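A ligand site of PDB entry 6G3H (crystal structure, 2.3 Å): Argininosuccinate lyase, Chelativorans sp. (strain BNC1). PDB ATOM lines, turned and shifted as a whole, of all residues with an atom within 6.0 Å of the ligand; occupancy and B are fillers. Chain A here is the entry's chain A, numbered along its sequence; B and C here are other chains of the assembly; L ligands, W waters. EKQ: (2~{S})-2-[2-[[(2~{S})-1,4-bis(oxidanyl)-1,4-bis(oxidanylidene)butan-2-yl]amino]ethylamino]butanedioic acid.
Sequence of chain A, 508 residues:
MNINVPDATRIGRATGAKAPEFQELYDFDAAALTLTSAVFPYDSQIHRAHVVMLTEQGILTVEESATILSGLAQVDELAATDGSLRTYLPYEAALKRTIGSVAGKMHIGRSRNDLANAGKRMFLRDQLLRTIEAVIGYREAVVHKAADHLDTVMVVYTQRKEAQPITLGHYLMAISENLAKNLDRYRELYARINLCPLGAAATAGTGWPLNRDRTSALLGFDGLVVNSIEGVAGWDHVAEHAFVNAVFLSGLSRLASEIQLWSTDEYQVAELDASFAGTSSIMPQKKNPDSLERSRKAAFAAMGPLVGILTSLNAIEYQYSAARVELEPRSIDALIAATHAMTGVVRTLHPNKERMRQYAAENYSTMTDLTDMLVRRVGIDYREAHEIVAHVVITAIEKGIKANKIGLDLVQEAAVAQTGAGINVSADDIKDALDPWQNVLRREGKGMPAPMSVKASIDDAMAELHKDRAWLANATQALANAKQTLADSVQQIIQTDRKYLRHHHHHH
O01 of the ligand is in salt-bridge range of NE of Arg 294.
OG of Ser 111 of chain B sits at hydrogen-bond distance from O14 of the ligand, at 2.5 Å.
The side-chain hydroxyl (OH) of Tyr 26 is in hydrogen-bond range of an oxygen (O03) of the ligand (2.6 Å).
The backbone NH of Ser 281 sits at hydrogen-bond distance from an oxygen (O13) of the ligand, 2.9 Å away.
O14 of the ligand sits at hydrogen-bond distance from OG of Ser 281, 2.7 Å away.
OG1 of Thr 158 of chain C is in hydrogen-bond range of O17 of the ligand, at 2.7 Å.
NZ of Lys 286 is in salt-bridge range of O16 of the ligand, 2.8 Å away.
O17 of the ligand lies within hydrogen-bond range of ND2 of Asn 113 of chain B (2.9 Å).
N of Arg 112 of chain B sits at hydrogen-bond distance from O14 of the ligand (2.9 Å).
The guanidinium group (NE) of Arg 112 of chain B is in salt-bridge range of an oxygen (O13) of the ligand.
An oxygen (O16) of the ligand sits at hydrogen-bond distance from the side-chain amide nitrogen (ND2) of Asn 288 (2.9 Å).
OG of Ser 280 sits close to O13 of the ligand (3.4 Å).
OD1 of Asp 290 is in salt-bridge range of N06 of the ligand.
The side-chain hydroxyl (OG) of Ser 111 of chain B sits at hydrogen-bond distance from the backbone NH (N) of Asn 113 of chain B (3.0 Å).
The side-chain amino group (NZ) of Lys 286 lies within hydrogen-bond range of the side-chain hydroxyl (OG1) of Thr 158 of chain C (2.6 Å).
NZ of Lys 286 is in hydrogen-bond range of OD1 of Asn 288 (2.8 Å).
OG1 of Thr 279 lies within hydrogen-bond range of O of Lys 286 (2.7 Å).
The backbone carbonyl oxygen of Tyr 320 of chain B sits at hydrogen-bond distance from the backbone NH of Gln 159 of chain C, 3.2 Å away.
O of Thr 279 sits close to ND2 of Asn 288 (3.4 Å).
The backbone NH (N) of Ile 282 sits close to the side-chain hydroxyl (OG) of Ser 280 (3.2 Å).
The side-chain hydroxyl (OG) of Ser 280 is in hydrogen-bond range of the backbone NH (N) of Met 283 (3.1 Å).
Merely in contact with the ligand: Gln 159 of chain C (2.8 Å), Ile 282 (3.3 Å), Met 283 (3.3 Å), Tyr 320 of chain B (3.4 Å) and Ala 322 of chain B (3.9 Å).
Hydrophobic or aromatic side chains that line the ligand: Tyr 26, Ile 282, Met 283, Tyr 320 of chain B and Ala 322 of chain B.
Within 4 Å of the ligand: Tyr 26, Ser 280, Ser 281, Ile 282, Met 283, Lys 286, Asn 288, Asp 290, Arg 294, Ser 111 of chain B, Arg 112 of chain B, Asn 113 of chain B, Tyr 320 of chain B, Ala 322 of chain B, Thr 158 of chain C and Gln 159 of chain C.
The nearest printed residue that does not touch the ligand is Thr 279 (4.3 Å).
Water W2 lies within hydrogen-bond range of the side-chain carboxylate of Asp 290, a nitrogen (N06) of the ligand, the side-chain amide nitrogen of Asn 288 and the backbone carbonyl oxygen of Thr 279.
Water W1 lies within hydrogen-bond range of OD1 of Asn 113 of chain B, O19 of the ligand, O of Arg 112 of chain B and OH of Tyr 320 of chain B.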
ATOM      1  N   TYR A  26       3.388  23.427 -18.709  1.00  0.00           N
ATOM      2  CA  TYR A  26       4.648  24.018 -19.133  1.00  0.00           C
ATOM      3  C   TYR A  26       4.680  25.535 -18.985  1.00  0.00           C
ATOM      4  O   TYR A  26       5.768  26.114 -19.005  1.00  0.00           O
ATOM      5  CB  TYR A  26       4.927  23.642 -20.592  1.00  0.00           C
ATOM      6  CG  TYR A  26       5.182  22.165 -20.779  1.00  0.00           C
ATOM      7  CD1 TYR A  26       4.125  21.270 -20.878  1.00  0.00           C
ATOM      8  CD2 TYR A  26       6.469  21.658 -20.808  1.00  0.00           C
ATOM      9  CE1 TYR A  26       4.343  19.921 -21.028  1.00  0.00           C
ATOM     10  CE2 TYR A  26       6.706  20.299 -20.952  1.00  0.00           C
ATOM     11  CZ  TYR A  26       5.634  19.435 -21.065  1.00  0.00           C
ATOM     12  OH  TYR A  26       5.863  18.092 -21.209  1.00  0.00           O
ATOM     13  N   THR A 279       7.048  12.391 -26.364  1.00  0.00           N
ATOM     14  CA  THR A 279       7.914  11.317 -26.841  1.00  0.00           C
ATOM     15  C   THR A 279       9.358  11.675 -26.532  1.00  0.00           C
ATOM     16  O   THR A 279       9.655  12.718 -25.946  1.00  0.00           O
ATOM     17  CB  THR A 279       7.710  11.052 -28.339  1.00  0.00           C
ATOM     18  OG1 THR A 279       8.481   9.917 -28.729  1.00  0.00           O
ATOM     19  CG2 THR A 279       8.115  12.277 -29.162  1.00  0.00           C
ATOM     20  N   SER A 280      10.261  10.798 -26.944  1.00  0.00           N
ATOM     21  CA  SER A 280      11.686  10.936 -26.681  1.00  0.00           C
ATOM     22  C   SER A 280      12.412  11.506 -27.883  1.00  0.00           C
ATOM     23  O   SER A 280      12.033  11.250 -29.041  1.00  0.00           O
ATOM     24  CB  SER A 280      12.292   9.583 -26.295  1.00  0.00           C
ATOM     25  OG  SER A 280      13.675   9.700 -26.014  1.00  0.00           O
ATOM     26  N   SER A 281      13.453  12.286 -27.618  1.00  0.00           N
ATOM     27  CA  SER A 281      14.314  12.802 -28.682  1.00  0.00           C
ATOM     28  C   SER A 281      15.247  11.744 -29.236  1.00  0.00           C
ATOM     29  O   SER A 281      15.859  11.970 -30.290  1.00  0.00           O
ATOM     30  CB  SER A 281      15.128  14.004 -28.169  1.00  0.00           C
ATOM     31  OG  SER A 281      15.999  13.635 -27.101  1.00  0.00           O
ATOM     32  N   ILE A 282      15.346  10.585 -28.590  1.00  0.00           N
ATOM     33  CA  ILE A 282      16.334   9.567 -28.922  1.00  0.00           C
ATOM     34  C   ILE A 282      15.632   8.225 -29.158  1.00  0.00           C
ATOM     35  O   ILE A 282      16.076   7.417 -29.980  1.00  0.00           O
ATOM     36  CB  ILE A 282      17.402   9.455 -27.817  1.00  0.00           C
ATOM     37  CG1 ILE A 282      18.329   8.269 -28.063  1.00  0.00           C
ATOM     38  CG2 ILE A 282      16.742   9.337 -26.441  1.00  0.00           C
ATOM     39  CD1 ILE A 282      19.559   8.262 -27.164  1.00  0.00           C
ATOM     40  N   MET A 283      14.534   7.989 -28.440  1.00  0.00           N
ATOM     41  CA  MET A 283      13.806   6.720 -28.512  1.00  0.00           C
ATOM     42  C   MET A 283      12.486   6.911 -29.257  1.00  0.00           C
ATOM     43  O   MET A 283      11.503   7.383 -28.656  1.00  0.00           O
ATOM     44  CB  MET A 283      13.540   6.184 -27.093  1.00  0.00           C
ATOM     45  CG  MET A 283      14.809   5.852 -26.321  1.00  0.00           C
ATOM     46  SD  MET A 283      14.525   5.318 -24.623  1.00  0.00           S
ATOM     47  CE  MET A 283      14.053   6.867 -23.858  1.00  0.00           C
ATOM     48  N   LYS A 286       8.788   5.881 -27.823  1.00  0.00           N
ATOM     49  CA  LYS A 286       8.232   6.410 -26.584  1.00  0.00           C
ATOM     50  C   LYS A 286       6.918   7.142 -26.825  1.00  0.00           C
ATOM     51  O   LYS A 286       6.823   8.008 -27.709  1.00  0.00           O
ATOM     52  CB  LYS A 286       9.221   7.352 -25.905  1.00  0.00           C
ATOM     53  CG  LYS A 286      10.357   6.660 -25.181  1.00  0.00           C
ATOM     54  CD  LYS A 286       9.841   5.696 -24.119  1.00  0.00           C
ATOM     55  CE  LYS A 286      10.725   5.709 -22.879  1.00  0.00           C
ATOM     56  NZ  LYS A 286      10.335   6.784 -21.924  1.00  0.00           N
ATOM     57  N   ASN A 288       5.225   9.167 -24.022  1.00  0.00           N
ATOM     58  CA  ASN A 288       5.648   9.465 -22.656  1.00  0.00           C
ATOM     59  C   ASN A 288       4.529  10.136 -21.862  1.00  0.00           C
ATOM     60  O   ASN A 288       3.922  11.093 -22.363  1.00  0.00           O
ATOM     61  CB  ASN A 288       6.878  10.365 -22.677  1.00  0.00           C
ATOM     62  CG  ASN A 288       8.140   9.611 -23.041  1.00  0.00           C
ATOM     63  OD1 ASN A 288       8.236   8.398 -22.821  1.00  0.00           O
ATOM     64  ND2 ASN A 288       9.112  10.309 -23.592  1.00  0.00           N
ATOM     65  N   ASP A 290       4.116  12.530 -19.928  1.00  0.00           N
ATOM     66  CA  ASP A 290       4.625  13.781 -19.390  1.00  0.00           C
ATOM     67  C   ASP A 290       3.547  14.517 -18.601  1.00  0.00           C
ATOM     68  O   ASP A 290       3.834  15.150 -17.575  1.00  0.00           O
ATOM     69  CB  ASP A 290       5.163  14.661 -20.518  1.00  0.00           C
ATOM     70  CG  ASP A 290       6.323  14.021 -21.237  1.00  0.00           C
ATOM     71  OD1 ASP A 290       7.063  13.240 -20.586  1.00  0.00           O
ATOM     72  OD2 ASP A 290       6.514  14.296 -22.442  1.00  0.00           O
ATOM     73  N   ARG A 294       4.228  15.435 -14.646  1.00  0.00           N
ATOM     74  CA  ARG A 294       4.264  16.837 -14.234  1.00  0.00           C
ATOM     75  C   ARG A 294       3.112  17.159 -13.291  1.00  0.00           C
ATOM     76  O   ARG A 294       3.224  18.072 -12.468  1.00  0.00           O
ATOM     77  CB  ARG A 294       4.230  17.749 -15.456  1.00  0.00           C
ATOM     78  CG  ARG A 294       5.597  17.967 -16.076  1.00  0.00           C
ATOM     79  CD  ARG A 294       5.545  18.882 -17.283  1.00  0.00           C
ATOM     80  NE  ARG A 294       6.883  19.128 -17.823  1.00  0.00           N
ATOM     81  CZ  ARG A 294       7.529  20.287 -17.792  1.00  0.00           C
ATOM     82  NH1 ARG A 294       6.984  21.368 -17.257  1.00  0.00           N
ATOM     83  NH2 ARG A 294       8.750  20.373 -18.313  1.00  0.00           N
ATOM     84  N   LEU B  89      14.709  20.733 -27.277  1.00  0.00           N
ATOM     85  CA  LEU B  89      14.178  20.446 -28.613  1.00  0.00           C
ATOM     86  C   LEU B  89      13.872  21.713 -29.391  1.00  0.00           C
ATOM     87  O   LEU B  89      14.257  21.793 -30.574  1.00  0.00           O
ATOM     88  CB  LEU B  89      12.953  19.533 -28.507  1.00  0.00           C
ATOM     89  CG  LEU B  89      13.241  18.030 -28.355  1.00  0.00           C
ATOM     90  CD1 LEU B  89      11.955  17.258 -28.146  1.00  0.00           C
ATOM     91  CD2 LEU B  89      13.988  17.472 -29.567  1.00  0.00           C
ATOM     92  N   HIS B 107      23.278  15.846 -31.203  1.00  0.00           N
ATOM     93  CA  HIS B 107      22.590  14.999 -30.234  1.00  0.00           C
ATOM     94  C   HIS B 107      22.993  13.535 -30.369  1.00  0.00           C
ATOM     95  O   HIS B 107      22.356  12.671 -29.745  1.00  0.00           O
ATOM     96  CB  HIS B 107      21.077  15.149 -30.394  1.00  0.00           C
ATOM     97  CG  HIS B 107      20.310  14.924 -29.129  1.00  0.00           C
ATOM     98  ND1 HIS B 107      20.747  15.381 -27.900  1.00  0.00           N
ATOM     99  CD2 HIS B 107      19.132  14.308 -28.902  1.00  0.00           C
ATOM    100  CE1 HIS B 107      19.883  15.034 -26.966  1.00  0.00           C
ATOM    101  NE2 HIS B 107      18.887  14.382 -27.549  1.00  0.00           N
ATOM    102  N   ARG B 110      23.340  10.998 -27.186  1.00  0.00           N
ATOM    103  CA  ARG B 110      22.916  11.860 -26.105  1.00  0.00           C
ATOM    104  C   ARG B 110      21.399  11.867 -26.029  1.00  0.00           C
ATOM    105  O   ARG B 110      20.705  11.501 -26.981  1.00  0.00           O
ATOM    106  CB  ARG B 110      23.466  13.286 -26.297  1.00  0.00           C
ATOM    107  CG  ARG B 110      23.201  14.218 -25.137  1.00  0.00           C
ATOM    108  CD  ARG B 110      23.877  15.566 -25.367  1.00  0.00           C
ATOM    109  NE  ARG B 110      23.221  16.315 -26.429  1.00  0.00           N
ATOM    110  CZ  ARG B 110      23.528  17.569 -26.761  1.00  0.00           C
ATOM    111  NH1 ARG B 110      24.496  18.205 -26.112  1.00  0.00           N
ATOM    112  NH2 ARG B 110      22.875  18.170 -27.744  1.00  0.00           N
ATOM    113  N   SER B 111      20.898  12.270 -24.864  1.00  0.00           N
ATOM    114  CA  SER B 111      19.477  12.331 -24.591  1.00  0.00           C
ATOM    115  C   SER B 111      19.186  13.663 -23.924  1.00  0.00           C
ATOM    116  O   SER B 111      20.098  14.381 -23.505  1.00  0.00           O
ATOM    117  CB  SER B 111      19.028  11.173 -23.695  1.00  0.00           C
ATOM    118  OG  SER B 111      17.702  11.359 -23.239  1.00  0.00           O
ATOM    119  N   ARG B 112      17.896  13.985 -23.807  1.00  0.00           N
ATOM    120  CA  ARG B 112      17.514  15.093 -22.945  1.00  0.00           C
ATOM    121  C   ARG B 112      17.720  14.747 -21.475  1.00  0.00           C
ATOM    122  O   ARG B 112      17.841  15.652 -20.645  1.00  0.00           O
ATOM    123  CB  ARG B 112      16.064  15.488 -23.199  1.00  0.00           C
ATOM    124  CG  ARG B 112      15.884  16.424 -24.396  1.00  0.00           C
ATOM    125  CD  ARG B 112      14.446  16.862 -24.580  1.00  0.00           C
ATOM    126  NE  ARG B 112      13.516  15.733 -24.659  1.00  0.00           N
ATOM    127  CZ  ARG B 112      12.196  15.837 -24.600  1.00  0.00           C
ATOM    128  NH1 ARG B 112      11.628  17.034 -24.455  1.00  0.00           N
ATOM    129  NH2 ARG B 112      11.428  14.761 -24.672  1.00  0.00           N
ATOM    130  N   ASN B 113      17.781  13.450 -21.144  1.00  0.00           N
ATOM    131  CA  ASN B 113      17.839  13.040 -19.746  1.00  0.00           C
ATOM    132  C   ASN B 113      19.212  13.310 -19.139  1.00  0.00           C
ATOM    133  O   ASN B 113      19.314  13.916 -18.070  1.00  0.00           O
ATOM    134  CB  ASN B 113      17.459  11.564 -19.617  1.00  0.00           C
ATOM    135  CG  ASN B 113      16.038  11.298 -20.071  1.00  0.00           C
ATOM    136  OD1 ASN B 113      15.249  12.228 -20.251  1.00  0.00           O
ATOM    137  ND2 ASN B 113      15.699  10.030 -20.239  1.00  0.00           N
ATOM    138  N   ALA B 202      19.880   8.151 -22.598  1.00  0.00           N
ATOM    139  CA  ALA B 202      18.557   8.083 -21.984  1.00  0.00           C
ATOM    140  C   ALA B 202      18.605   7.489 -20.582  1.00  0.00           C
ATOM    141  O   ALA B 202      17.814   7.888 -19.720  1.00  0.00           O
ATOM    142  CB  ALA B 202      17.612   7.265 -22.860  1.00  0.00           C
ATOM    143  N   TYR B 320      14.912   7.544 -14.586  1.00  0.00           N
ATOM    144  CA  TYR B 320      14.605   8.915 -14.961  1.00  0.00           C
ATOM    145  C   TYR B 320      13.125   9.142 -14.742  1.00  0.00           C
ATOM    146  O   TYR B 320      12.302   8.257 -14.982  1.00  0.00           O
ATOM    147  CB  TYR B 320      14.961   9.208 -16.414  1.00  0.00           C
ATOM    148  CG  TYR B 320      14.424  10.564 -16.834  1.00  0.00           C
ATOM    149  CD1 TYR B 320      13.126  10.694 -17.317  1.00  0.00           C
ATOM    150  CD2 TYR B 320      15.189  11.707 -16.685  1.00  0.00           C
ATOM    151  CE1 TYR B 320      12.616  11.926 -17.659  1.00  0.00           C
ATOM    152  CE2 TYR B 320      14.689  12.945 -17.035  1.00  0.00           C
ATOM    153  CZ  TYR B 320      13.396  13.045 -17.518  1.00  0.00           C
ATOM    154  OH  TYR B 320      12.895  14.275 -17.876  1.00  0.00           O
ATOM    155  N   ALA B 322      10.204  12.647 -14.864  1.00  0.00           N
ATOM    156  CA  ALA B 322       9.866  14.052 -14.932  1.00  0.00           C
ATOM    157  C   ALA B 322       8.994  14.486 -13.766  1.00  0.00           C
ATOM    158  O   ALA B 322       8.576  15.650 -13.710  1.00  0.00           O
ATOM    159  CB  ALA B 322       9.181  14.377 -16.263  1.00  0.00           C
ATOM    160  N   THR C 158      12.208   4.520 -18.509  1.00  0.00           N
ATOM    161  CA  THR C 158      12.139   5.916 -18.124  1.00  0.00           C
ATOM    162  C   THR C 158      10.669   6.335 -18.164  1.00  0.00           C
ATOM    163  O   THR C 158       9.951   6.016 -19.115  1.00  0.00           O
ATOM    164  CB  THR C 158      12.962   6.821 -19.042  1.00  0.00           C
ATOM    165  OG1 THR C 158      12.434   6.792 -20.367  1.00  0.00           O
ATOM    166  CG2 THR C 158      14.435   6.379 -19.052  1.00  0.00           C
ATOM    167  N   GLN C 159      10.246   7.031 -17.116  1.00  0.00           N
ATOM    168  CA  GLN C 159       8.841   7.437 -16.955  1.00  0.00           C
ATOM    169  C   GLN C 159       7.910   6.230 -17.011  1.00  0.00           C
ATOM    170  O   GLN C 159       6.818   6.296 -17.582  1.00  0.00           O
ATOM    171  CB  GLN C 159       8.442   8.461 -18.014  1.00  0.00           C
ATOM    172  CG  GLN C 159       9.453   9.555 -18.253  1.00  0.00           C
ATOM    173  CD  GLN C 159       8.905  10.643 -19.152  1.00  0.00           C
ATOM    174  OE1 GLN C 159       9.178  10.669 -20.352  1.00  0.00           O
ATOM    175  NE2 GLN C 159       8.099  11.538 -18.578  1.00  0.00           N
ATOM    176  N   ALA C 163      12.419   1.789 -22.274  1.00  0.00           N
ATOM    177  CA  ALA C 163      13.333   2.730 -22.901  1.00  0.00           C
ATOM    178  C   ALA C 163      14.311   2.007 -23.810  1.00  0.00           C
ATOM    179  O   ALA C 163      14.246   2.150 -25.034  1.00  0.00           O
ATOM    180  CB  ALA C 163      14.076   3.521 -21.816  1.00  0.00           C
HETATM  181  C10 EKQ L   1      13.024  10.942 -22.967  1.00  0.00           C
HETATM  182  C15 EKQ L   1      12.613   9.598 -22.355  1.00  0.00           C
HETATM  183  O01 EKQ L   1       8.330  17.335 -18.721  1.00  0.00           O
HETATM  184  C02 EKQ L   1       8.686  16.932 -19.924  1.00  0.00           C
HETATM  185  O03 EKQ L   1       8.359  17.488 -20.926  1.00  0.00           O
HETATM  186  C04 EKQ L   1       9.555  15.698 -19.916  1.00  0.00           C
HETATM  187  C05 EKQ L   1      10.466  15.658 -21.134  1.00  0.00           C
HETATM  188  N06 EKQ L   1      10.721  14.245 -21.576  1.00  0.00           N
HETATM  189  C07 EKQ L   1      11.093  13.246 -20.523  1.00  0.00           C
HETATM  190  C08 EKQ L   1      11.600  11.941 -21.080  1.00  0.00           C
HETATM  191  N09 EKQ L   1      12.793  12.036 -21.968  1.00  0.00           N
HETATM  192  C11 EKQ L   1      14.464  10.980 -23.449  1.00  0.00           C
HETATM  193  C12 EKQ L   1      14.694  12.085 -24.440  1.00  0.00           C
HETATM  194  O13 EKQ L   1      13.832  12.830 -24.775  1.00  0.00           O
HETATM  195  O14 EKQ L   1      15.927  12.143 -24.890  1.00  0.00           O
HETATM  196  O16 EKQ L   1      11.659   9.011 -22.928  1.00  0.00           O
HETATM  197  O17 EKQ L   1      13.215   9.178 -21.356  1.00  0.00           O
HETATM  198  C18 EKQ L   1      11.807  16.360 -20.906  1.00  0.00           C
HETATM  199  O19 EKQ L   1      12.816  15.808 -21.401  1.00  0.00           O
HETATM  200  O20 EKQ L   1      11.806  17.409 -20.238  1.00  0.00           O
HETATM  201  O   HOH W   1      15.077  14.907 -19.924  1.00  0.00           O
HETATM  202  O   HOH W   2       8.628  13.106 -23.077  1.00  0.00           O
